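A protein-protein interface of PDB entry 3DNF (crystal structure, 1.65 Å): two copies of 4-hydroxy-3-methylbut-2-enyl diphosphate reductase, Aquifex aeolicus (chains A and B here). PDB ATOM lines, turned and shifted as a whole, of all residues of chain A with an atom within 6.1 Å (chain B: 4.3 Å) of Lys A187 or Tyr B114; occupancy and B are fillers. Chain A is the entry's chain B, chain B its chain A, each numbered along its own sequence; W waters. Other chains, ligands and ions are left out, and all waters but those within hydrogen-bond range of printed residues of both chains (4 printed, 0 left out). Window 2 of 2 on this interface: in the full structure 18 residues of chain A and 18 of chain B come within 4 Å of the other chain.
NZ of Lys B187 lies within salt-bridge range of OE1 of Glu B112, at 2.7 Å. The side-chain carboxylate of Glu A112 is in salt-bridge range of the side-chain amino group of Lys A187. The backbone NH of Tyr B114 is in hydrogen-bond range of the backbone carbonyl oxygen of Leu B109 (3.0 Å). N of Lys B187 is in hydrogen-bond range of O of Val B159, 2.9 Å away. The backbone NH of Lys A187 is in hydrogen-bond range of the backbone carbonyl oxygen of Val A159 (2.9 Å). The backbone NH (N) of Ile A161 is in hydrogen-bond range of the backbone carbonyl oxygen (O) of Lys A187 (2.7 Å).
The side-chain carboxylate (OE2) of Glu B185 lies within salt-bridge range of the side-chain amino group (NZ) of Lys A187 (3.2 Å). The side-chain carboxylate (OE2) of Glu A185 lies within salt-bridge range of the side-chain amino group (NZ) of Lys B187 (3.1 Å). The backbone carbonyl oxygen (O) of Val B186 sits at hydrogen-bond distance from the backbone NH (N) of Val A188.
Tyr A114 touches Lys B187, and with the chains exchanged Lys A187 touches Tyr B114. Glu A185 touches Lys B187, and with the chains exchanged Lys A187 touches Glu B185. Val B186 touches its own counterpart, Val A186. Val A186 touches Lys B187, and with the chains exchanged Lys A187 touches Val B186. 8 positions are printed for both chains.
Water W1 bridges OE1 of Glu A185 and NZ of Lys B187. Water W4 lies within hydrogen-bond range of OH of Tyr A114 (2.6 Å) and NZ of Lys B187 (2.9 Å). Water W3 bridges the side-chain hydroxyl of Tyr B114 (2.6 Å) and the side-chain amino group of Lys A187 (3.0 Å). Water W2 lies within hydrogen-bond range of the side-chain amide nitrogen of Gln A108 (2.7 Å), the side-chain carboxylate of Glu B185 (2.9 Å) and the side-chain amino group of Lys A187 (3.1 Å).
Of the printed residues of chain B, Lys A187 touches Tyr B114 (3.8 Å), Glu B185 (3.1 Å) and Val B186 (3.3 Å). Tyr B114 touches just one residue of chain A: Lys A187. Of the printed residues of chain A, Val B186 touches Val A186 (3.8 Å), Lys A187 (3.3 Å) and Val A188 (2.7 Å). Printed residues of chain B within 4 Å of Glu A185: Lys B187 (3.0 Å). Of the printed residues of chain A, Lys B187 touches Tyr A114 (3.7 Å), Glu A185 (3.0 Å) and Val A186 (3.3 Å). Gln A108 touches none of the printed residues of chain B. The nearest printed residue of chain B that does not touch Val A186 is Tyr B114 (6.8 Å).
Among the printed residues, pairs that only touch across the chains: Tyr A114 with Lys B187 (3.7 Å), Val A186 with Val B186 (3.8 Å), Val A186 with Lys B187 (3.3 Å), Lys A187 with Tyr B114 (3.8 Å), Lys A187 with Val B186 (3.3 Å) and Val A188 with Glu B185 (3.2 Å).
Hydrophobic or aromatic side chains of chain A that line the printed part of chain B: Tyr A114 and Val A188. Of the 13 printed residues of chain B, 4 touch a printed residue of chain A. Printed residues of chain B that touch a printed residue of chain A: Tyr B114, Glu B185, Val B186 and Lys B187. Among the printed residues, Asp or Glu carboxylates within 4 Å of a Lys or Arg side-chain nitrogen of the other chain: Glu A185 with Lys B187 (3.1 Å) and Lys A187 with Glu B185 (3.2 Å).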
ATOM      1  N   GLN A 108      -7.125  -0.859   3.721  1.00  0.00           N
ATOM      2  CA  GLN A 108      -8.466  -1.401   3.591  1.00  0.00           C
ATOM      3  C   GLN A 108      -8.417  -2.913   3.448  1.00  0.00           C
ATOM      4  O   GLN A 108      -9.134  -3.600   4.172  1.00  0.00           O
ATOM      5  CB  GLN A 108      -9.208  -0.751   2.431  1.00  0.00           C
ATOM      6  CG  GLN A 108     -10.614  -1.316   2.238  1.00  0.00           C
ATOM      7  CD  GLN A 108     -11.156  -1.009   0.862  1.00  0.00           C
ATOM      8  OE1 GLN A 108     -10.680  -0.096   0.185  1.00  0.00           O
ATOM      9  NE2 GLN A 108     -12.143  -1.770   0.440  1.00  0.00           N
ATOM     10  N   LEU A 109      -7.564  -3.425   2.535  1.00  0.00           N
ATOM     11  CA  LEU A 109      -7.435  -4.845   2.331  1.00  0.00           C
ATOM     12  C   LEU A 109      -6.974  -5.569   3.611  1.00  0.00           C
ATOM     13  O   LEU A 109      -7.452  -6.675   3.919  1.00  0.00           O
ATOM     14  CB  LEU A 109      -6.487  -5.127   1.147  1.00  0.00           C
ATOM     15  CG  LEU A 109      -7.029  -4.812  -0.276  1.00  0.00           C
ATOM     16  CD1 LEU A 109      -5.884  -4.972  -1.290  1.00  0.00           C
ATOM     17  CD2 LEU A 109      -8.209  -5.706  -0.682  1.00  0.00           C
ATOM     18  N   GLU A 112      -9.792  -5.959   6.005  1.00  0.00           N
ATOM     19  CA  GLU A 112     -10.693  -6.971   5.491  1.00  0.00           C
ATOM     20  C   GLU A 112     -10.087  -8.381   5.564  1.00  0.00           C
ATOM     21  O   GLU A 112     -10.745  -9.320   5.190  1.00  0.00           O
ATOM     22  CB  GLU A 112     -11.128  -6.599   4.060  1.00  0.00           C
ATOM     23  CG  GLU A 112     -11.927  -5.253   4.000  1.00  0.00           C
ATOM     24  CD  GLU A 112     -12.257  -4.779   2.573  1.00  0.00           C
ATOM     25  OE1 GLU A 112     -11.748  -5.381   1.610  1.00  0.00           O
ATOM     26  OE2 GLU A 112     -13.015  -3.788   2.404  1.00  0.00           O
ATOM     27  N   TYR A 114      -7.118  -9.596   4.234  1.00  0.00           N
ATOM     28  CA  TYR A 114      -6.336 -10.134   3.099  1.00  0.00           C
ATOM     29  C   TYR A 114      -4.823 -10.074   3.291  1.00  0.00           C
ATOM     30  O   TYR A 114      -4.313  -9.159   3.955  1.00  0.00           O
ATOM     31  CB  TYR A 114      -6.627  -9.372   1.783  1.00  0.00           C
ATOM     32  CG  TYR A 114      -8.022  -9.575   1.270  1.00  0.00           C
ATOM     33  CD1 TYR A 114      -8.331 -10.665   0.475  1.00  0.00           C
ATOM     34  CD2 TYR A 114      -9.070  -8.697   1.644  1.00  0.00           C
ATOM     35  CE1 TYR A 114      -9.634 -10.869   0.023  1.00  0.00           C
ATOM     36  CE2 TYR A 114     -10.362  -8.886   1.194  1.00  0.00           C
ATOM     37  CZ  TYR A 114     -10.642  -9.984   0.381  1.00  0.00           C
ATOM     38  OH  TYR A 114     -11.914 -10.188  -0.054  1.00  0.00           O
ATOM     39  N   VAL A 159      -6.286 -13.373  -0.827  1.00  0.00           N
ATOM     40  CA  VAL A 159      -5.242 -12.486  -1.314  1.00  0.00           C
ATOM     41  C   VAL A 159      -5.864 -11.219  -1.893  1.00  0.00           C
ATOM     42  O   VAL A 159      -6.789 -11.296  -2.692  1.00  0.00           O
ATOM     43  CB  VAL A 159      -4.283 -13.146  -2.367  1.00  0.00           C
ATOM     44  CG1 VAL A 159      -3.299 -12.116  -2.937  1.00  0.00           C
ATOM     45  CG2 VAL A 159      -3.548 -14.332  -1.757  1.00  0.00           C
ATOM     46  N   GLY A 160      -5.386 -10.062  -1.416  1.00  0.00           N
ATOM     47  CA  GLY A 160      -5.769  -8.766  -2.000  1.00  0.00           C
ATOM     48  C   GLY A 160      -4.674  -8.200  -2.875  1.00  0.00           C
ATOM     49  O   GLY A 160      -3.507  -8.091  -2.460  1.00  0.00           O
ATOM     50  N   ILE A 161      -5.062  -7.714  -4.071  1.00  0.00           N
ATOM     51  CA  ILE A 161      -4.091  -7.312  -5.040  1.00  0.00           C
ATOM     52  C   ILE A 161      -4.260  -5.852  -5.412  1.00  0.00           C
ATOM     53  O   ILE A 161      -5.375  -5.437  -5.769  1.00  0.00           O
ATOM     54  CB  ILE A 161      -4.142  -8.220  -6.307  1.00  0.00           C
ATOM     55  CG1 ILE A 161      -3.989  -9.668  -5.870  1.00  0.00           C
ATOM     56  CG2 ILE A 161      -3.062  -7.850  -7.353  1.00  0.00           C
ATOM     57  CD1 ILE A 161      -4.229 -10.683  -6.978  1.00  0.00           C
ATOM     58  N   VAL A 162      -3.154  -5.111  -5.294  1.00  0.00           N
ATOM     59  CA  VAL A 162      -3.109  -3.720  -5.766  1.00  0.00           C
ATOM     60  C   VAL A 162      -1.921  -3.526  -6.738  1.00  0.00           C
ATOM     61  O   VAL A 162      -1.122  -4.456  -6.959  1.00  0.00           O
ATOM     62  CB  VAL A 162      -3.045  -2.700  -4.603  1.00  0.00           C
ATOM     63  CG1 VAL A 162      -4.317  -2.818  -3.768  1.00  0.00           C
ATOM     64  CG2 VAL A 162      -1.785  -2.875  -3.794  1.00  0.00           C
ATOM     65  N   GLU A 185      -9.951 -17.023  -2.599  1.00  0.00           N
ATOM     66  CA  GLU A 185     -10.618 -15.753  -2.697  1.00  0.00           C
ATOM     67  C   GLU A 185      -9.619 -14.648  -2.987  1.00  0.00           C
ATOM     68  O   GLU A 185      -8.623 -14.486  -2.291  1.00  0.00           O
ATOM     69  CB  GLU A 185     -11.387 -15.476  -1.410  1.00  0.00           C
ATOM     70  CG  GLU A 185     -11.916 -14.111  -1.333  1.00  0.00           C
ATOM     71  CD  GLU A 185     -12.735 -13.870  -0.095  1.00  0.00           C
ATOM     72  OE1 GLU A 185     -13.435 -14.801   0.375  1.00  0.00           O
ATOM     73  OE2 GLU A 185     -12.685 -12.722   0.392  1.00  0.00           O
ATOM     74  N   VAL A 186      -9.888 -13.897  -4.053  1.00  0.00           N
ATOM     75  CA  VAL A 186      -8.977 -12.843  -4.438  1.00  0.00           C
ATOM     76  C   VAL A 186      -9.782 -11.553  -4.517  1.00  0.00           C
ATOM     77  O   VAL A 186     -10.848 -11.538  -5.114  1.00  0.00           O
ATOM     78  CB  VAL A 186      -8.316 -13.107  -5.815  1.00  0.00           C
ATOM     79  CG1 VAL A 186      -7.537 -11.854  -6.262  1.00  0.00           C
ATOM     80  CG2 VAL A 186      -7.389 -14.295  -5.719  1.00  0.00           C
ATOM     81  N   LYS A 187      -9.264 -10.467  -3.937  1.00  0.00           N
ATOM     82  CA  LYS A 187      -9.873  -9.167  -4.154  1.00  0.00           C
ATOM     83  C   LYS A 187      -8.875  -8.243  -4.824  1.00  0.00           C
ATOM     84  O   LYS A 187      -7.742  -8.128  -4.385  1.00  0.00           O
ATOM     85  CB  LYS A 187     -10.374  -8.541  -2.843  1.00  0.00           C
ATOM     86  CG  LYS A 187     -10.923  -7.134  -3.003  1.00  0.00           C
ATOM     87  CD  LYS A 187     -11.724  -6.751  -1.778  1.00  0.00           C
ATOM     88  CE  LYS A 187     -12.125  -5.296  -1.765  1.00  0.00           C
ATOM     89  NZ  LYS A 187     -13.105  -5.065  -0.652  1.00  0.00           N
ATOM     90  N   VAL A 188      -9.295  -7.591  -5.905  1.00  0.00           N
ATOM     91  CA  VAL A 188      -8.417  -6.703  -6.621  1.00  0.00           C
ATOM     92  C   VAL A 188      -8.946  -5.302  -6.544  1.00  0.00           C
ATOM     93  O   VAL A 188     -10.124  -5.048  -6.810  1.00  0.00           O
ATOM     94  CB  VAL A 188      -8.363  -7.080  -8.133  1.00  0.00           C
ATOM     95  CG1 VAL A 188      -7.411  -6.161  -8.941  1.00  0.00           C
ATOM     96  CG2 VAL A 188      -8.034  -8.562  -8.301  1.00  0.00           C
ATOM     97  N   ILE A 189      -8.077  -4.390  -6.108  1.00  0.00           N
ATOM     98  CA  ILE A 189      -8.401  -2.983  -6.251  1.00  0.00           C
ATOM     99  C   ILE A 189      -7.422  -2.414  -7.283  1.00  0.00           C
ATOM    100  O   ILE A 189      -6.207  -2.280  -7.025  1.00  0.00           O
ATOM    101  CB  ILE A 189      -8.308  -2.248  -4.909  1.00  0.00           C
ATOM    102  CG1 ILE A 189      -9.273  -2.891  -3.902  1.00  0.00           C
ATOM    103  CG2 ILE A 189      -8.556  -0.702  -5.152  1.00  0.00           C
ATOM    104  CD1 ILE A 189      -9.065  -2.369  -2.471  1.00  0.00           C
ATOM    105  N   LEU B 109     -21.484 -12.781  -2.353  1.00  0.00           N
ATOM    106  CA  LEU B 109     -21.135 -11.623  -3.156  1.00  0.00           C
ATOM    107  C   LEU B 109     -22.235 -10.569  -3.220  1.00  0.00           C
ATOM    108  O   LEU B 109     -21.935  -9.368  -3.231  1.00  0.00           O
ATOM    109  CB  LEU B 109     -20.719 -12.063  -4.552  1.00  0.00           C
ATOM    110  CG  LEU B 109     -19.383 -12.809  -4.568  1.00  0.00           C
ATOM    111  CD1 LEU B 109     -19.166 -13.595  -5.873  1.00  0.00           C
ATOM    112  CD2 LEU B 109     -18.063 -11.985  -4.178  1.00  0.00           C
ATOM    113  N   THR B 110     -23.495 -10.991  -3.322  1.00  0.00           N
ATOM    114  CA  THR B 110     -24.624 -10.093  -3.367  1.00  0.00           C
ATOM    115  C   THR B 110     -24.683  -9.374  -2.047  1.00  0.00           C
ATOM    116  O   THR B 110     -24.868  -8.163  -2.016  1.00  0.00           O
ATOM    117  CB  THR B 110     -25.928 -10.884  -3.620  1.00  0.00           C
ATOM    118  OG1 THR B 110     -25.877 -11.405  -4.955  1.00  0.00           O
ATOM    119  CG2 THR B 110     -27.127 -10.054  -3.480  1.00  0.00           C
ATOM    120  N   GLU B 112     -22.358  -8.636  -0.114  1.00  0.00           N
ATOM    121  CA  GLU B 112     -21.190  -7.764  -0.018  1.00  0.00           C
ATOM    122  C   GLU B 112     -21.265  -6.617  -1.037  1.00  0.00           C
ATOM    123  O   GLU B 112     -20.322  -5.829  -1.133  1.00  0.00           O
ATOM    124  CB  GLU B 112     -19.931  -8.590  -0.282  1.00  0.00           C
ATOM    125  CG  GLU B 112     -19.614  -9.522   0.936  1.00  0.00           C
ATOM    126  CD  GLU B 112     -18.481 -10.503   0.687  1.00  0.00           C
ATOM    127  OE1 GLU B 112     -17.897 -10.539  -0.424  1.00  0.00           O
ATOM    128  OE2 GLU B 112     -18.137 -11.239   1.667  1.00  0.00           O
ATOM    129  N   GLY B 113     -22.334  -6.606  -1.827  1.00  0.00           N
ATOM    130  CA  GLY B 113     -22.627  -5.514  -2.789  1.00  0.00           C
ATOM    131  C   GLY B 113     -21.991  -5.584  -4.186  1.00  0.00           C
ATOM    132  O   GLY B 113     -21.838  -4.518  -4.855  1.00  0.00           O
ATOM    133  N   TYR B 114     -21.699  -6.786  -4.656  1.00  0.00           N
ATOM    134  CA  TYR B 114     -21.131  -7.007  -5.984  1.00  0.00           C
ATOM    135  C   TYR B 114     -22.164  -7.337  -7.053  1.00  0.00           C
ATOM    136  O   TYR B 114     -23.147  -8.002  -6.772  1.00  0.00           O
ATOM    137  CB  TYR B 114     -20.167  -8.184  -5.944  1.00  0.00           C
ATOM    138  CG  TYR B 114     -18.923  -7.892  -5.170  1.00  0.00           C
ATOM    139  CD1 TYR B 114     -17.872  -7.178  -5.757  1.00  0.00           C
ATOM    140  CD2 TYR B 114     -18.783  -8.314  -3.821  1.00  0.00           C
ATOM    141  CE1 TYR B 114     -16.702  -6.871  -5.044  1.00  0.00           C
ATOM    142  CE2 TYR B 114     -17.634  -8.004  -3.111  1.00  0.00           C
ATOM    143  CZ  TYR B 114     -16.595  -7.295  -3.727  1.00  0.00           C
ATOM    144  OH  TYR B 114     -15.460  -6.979  -3.008  1.00  0.00           O
ATOM    145  N   PHE B 115     -21.950  -6.821  -8.265  1.00  0.00           N
ATOM    146  CA  PHE B 115     -22.664  -7.285  -9.430  1.00  0.00           C
ATOM    147  C   PHE B 115     -21.961  -8.598  -9.808  1.00  0.00           C
ATOM    148  O   PHE B 115     -20.743  -8.640  -9.892  1.00  0.00           O
ATOM    149  CB  PHE B 115     -22.536  -6.250 -10.552  1.00  0.00           C
ATOM    150  CG  PHE B 115     -23.147  -6.703 -11.850  1.00  0.00           C
ATOM    151  CD1 PHE B 115     -24.478  -6.457 -12.115  1.00  0.00           C
ATOM    152  CD2 PHE B 115     -22.394  -7.448 -12.775  1.00  0.00           C
ATOM    153  CE1 PHE B 115     -25.082  -6.851 -13.352  1.00  0.00           C
ATOM    154  CE2 PHE B 115     -22.984  -7.864 -13.991  1.00  0.00           C
ATOM    155  CZ  PHE B 115     -24.309  -7.581 -14.271  1.00  0.00           C
ATOM    156  N   VAL B 116     -22.723  -9.660 -10.060  1.00  0.00           N
ATOM    157  CA  VAL B 116     -22.122 -10.955 -10.160  1.00  0.00           C
ATOM    158  C   VAL B 116     -21.894 -11.435 -11.582  1.00  0.00           C
ATOM    159  O   VAL B 116     -22.801 -11.420 -12.419  1.00  0.00           O
ATOM    160  CB  VAL B 116     -22.963 -12.035  -9.405  1.00  0.00           C
ATOM    161  CG1 VAL B 116     -22.330 -13.358  -9.572  1.00  0.00           C
ATOM    162  CG2 VAL B 116     -23.011 -11.725  -7.914  1.00  0.00           C
ATOM    163  N   ARG B 158     -18.008  -2.506  -8.897  1.00  0.00           N
ATOM    164  CA  ARG B 158     -17.663  -3.678  -8.046  1.00  0.00           C
ATOM    165  C   ARG B 158     -18.255  -4.957  -8.612  1.00  0.00           C
ATOM    166  O   ARG B 158     -19.471  -5.142  -8.599  1.00  0.00           O
ATOM    167  CB  ARG B 158     -18.132  -3.462  -6.606  1.00  0.00           C
ATOM    168  CG  ARG B 158     -17.590  -2.165  -6.018  1.00  0.00           C
ATOM    169  CD  ARG B 158     -18.140  -1.924  -4.620  1.00  0.00           C
ATOM    170  NE  ARG B 158     -17.437  -2.759  -3.665  1.00  0.00           N
ATOM    171  CZ  ARG B 158     -18.001  -3.577  -2.791  1.00  0.00           C
ATOM    172  NH1 ARG B 158     -19.323  -3.654  -2.695  1.00  0.00           N
ATOM    173  NH2 ARG B 158     -17.233  -4.285  -1.982  1.00  0.00           N
ATOM    174  N   VAL B 159     -17.385  -5.790  -9.181  1.00  0.00           N
ATOM    175  CA  VAL B 159     -17.816  -7.032  -9.813  1.00  0.00           C
ATOM    176  C   VAL B 159     -17.311  -8.249  -9.013  1.00  0.00           C
ATOM    177  O   VAL B 159     -16.129  -8.310  -8.642  1.00  0.00           O
ATOM    178  CB  VAL B 159     -17.346  -7.093 -11.285  1.00  0.00           C
ATOM    179  CG1 VAL B 159     -17.698  -8.450 -11.928  1.00  0.00           C
ATOM    180  CG2 VAL B 159     -17.978  -5.956 -12.099  1.00  0.00           C
ATOM    181  N   GLY B 160     -18.220  -9.184  -8.723  1.00  0.00           N
ATOM    182  CA  GLY B 160     -17.862 -10.446  -8.021  1.00  0.00           C
ATOM    183  C   GLY B 160     -17.937 -11.574  -9.047  1.00  0.00           C
ATOM    184  O   GLY B 160     -18.956 -11.695  -9.761  1.00  0.00           O
ATOM    185  N   GLU B 185     -13.059  -2.538  -8.699  1.00  0.00           N
ATOM    186  CA  GLU B 185     -12.864  -3.554  -7.679  1.00  0.00           C
ATOM    187  C   GLU B 185     -13.458  -4.833  -8.145  1.00  0.00           C
ATOM    188  O   GLU B 185     -14.595  -4.843  -8.608  1.00  0.00           O
ATOM    189  CB  GLU B 185     -13.589  -3.117  -6.413  1.00  0.00           C
ATOM    190  CG  GLU B 185     -13.516  -4.104  -5.279  1.00  0.00           C
ATOM    191  CD  GLU B 185     -14.310  -3.654  -4.075  1.00  0.00           C
ATOM    192  OE1 GLU B 185     -14.491  -2.435  -3.901  1.00  0.00           O
ATOM    193  OE2 GLU B 185     -14.753  -4.515  -3.287  1.00  0.00           O
ATOM    194  N   VAL B 186     -12.696  -5.916  -7.995  1.00  0.00           N
ATOM    195  CA  VAL B 186     -13.141  -7.250  -8.418  1.00  0.00           C
ATOM    196  C   VAL B 186     -12.921  -8.179  -7.251  1.00  0.00           C
ATOM    197  O   VAL B 186     -11.880  -8.157  -6.624  1.00  0.00           O
ATOM    198  CB  VAL B 186     -12.355  -7.723  -9.678  1.00  0.00           C
ATOM    199  CG1 VAL B 186     -12.637  -9.161 -10.023  1.00  0.00           C
ATOM    200  CG2 VAL B 186     -12.670  -6.851 -10.879  1.00  0.00           C
ATOM    201  N   LYS B 187     -13.924  -8.979  -6.949  1.00  0.00           N
ATOM    202  CA  LYS B 187     -13.666 -10.069  -5.993  1.00  0.00           C
ATOM    203  C   LYS B 187     -13.951 -11.376  -6.694  1.00  0.00           C
ATOM    204  O   LYS B 187     -15.045 -11.525  -7.284  1.00  0.00           O
ATOM    205  CB  LYS B 187     -14.558  -9.969  -4.781  1.00  0.00           C
ATOM    206  CG  LYS B 187     -14.243 -11.083  -3.722  1.00  0.00           C
ATOM    207  CD  LYS B 187     -14.975 -10.778  -2.442  1.00  0.00           C
ATOM    208  CE  LYS B 187     -14.857 -11.932  -1.444  1.00  0.00           C
ATOM    209  NZ  LYS B 187     -15.407 -11.417  -0.129  1.00  0.00           N
HETATM  210  O   HOH W   1     -15.239 -13.638   1.713  1.00  0.00           O
HETATM  211  O   HOH W   2     -14.309  -2.246  -1.059  1.00  0.00           O
HETATM  212  O   HOH W   3     -15.384  -6.990  -0.395  1.00  0.00           O
HETATM  213  O   HOH W   4     -14.075  -9.074   0.848  1.00  0.00           O
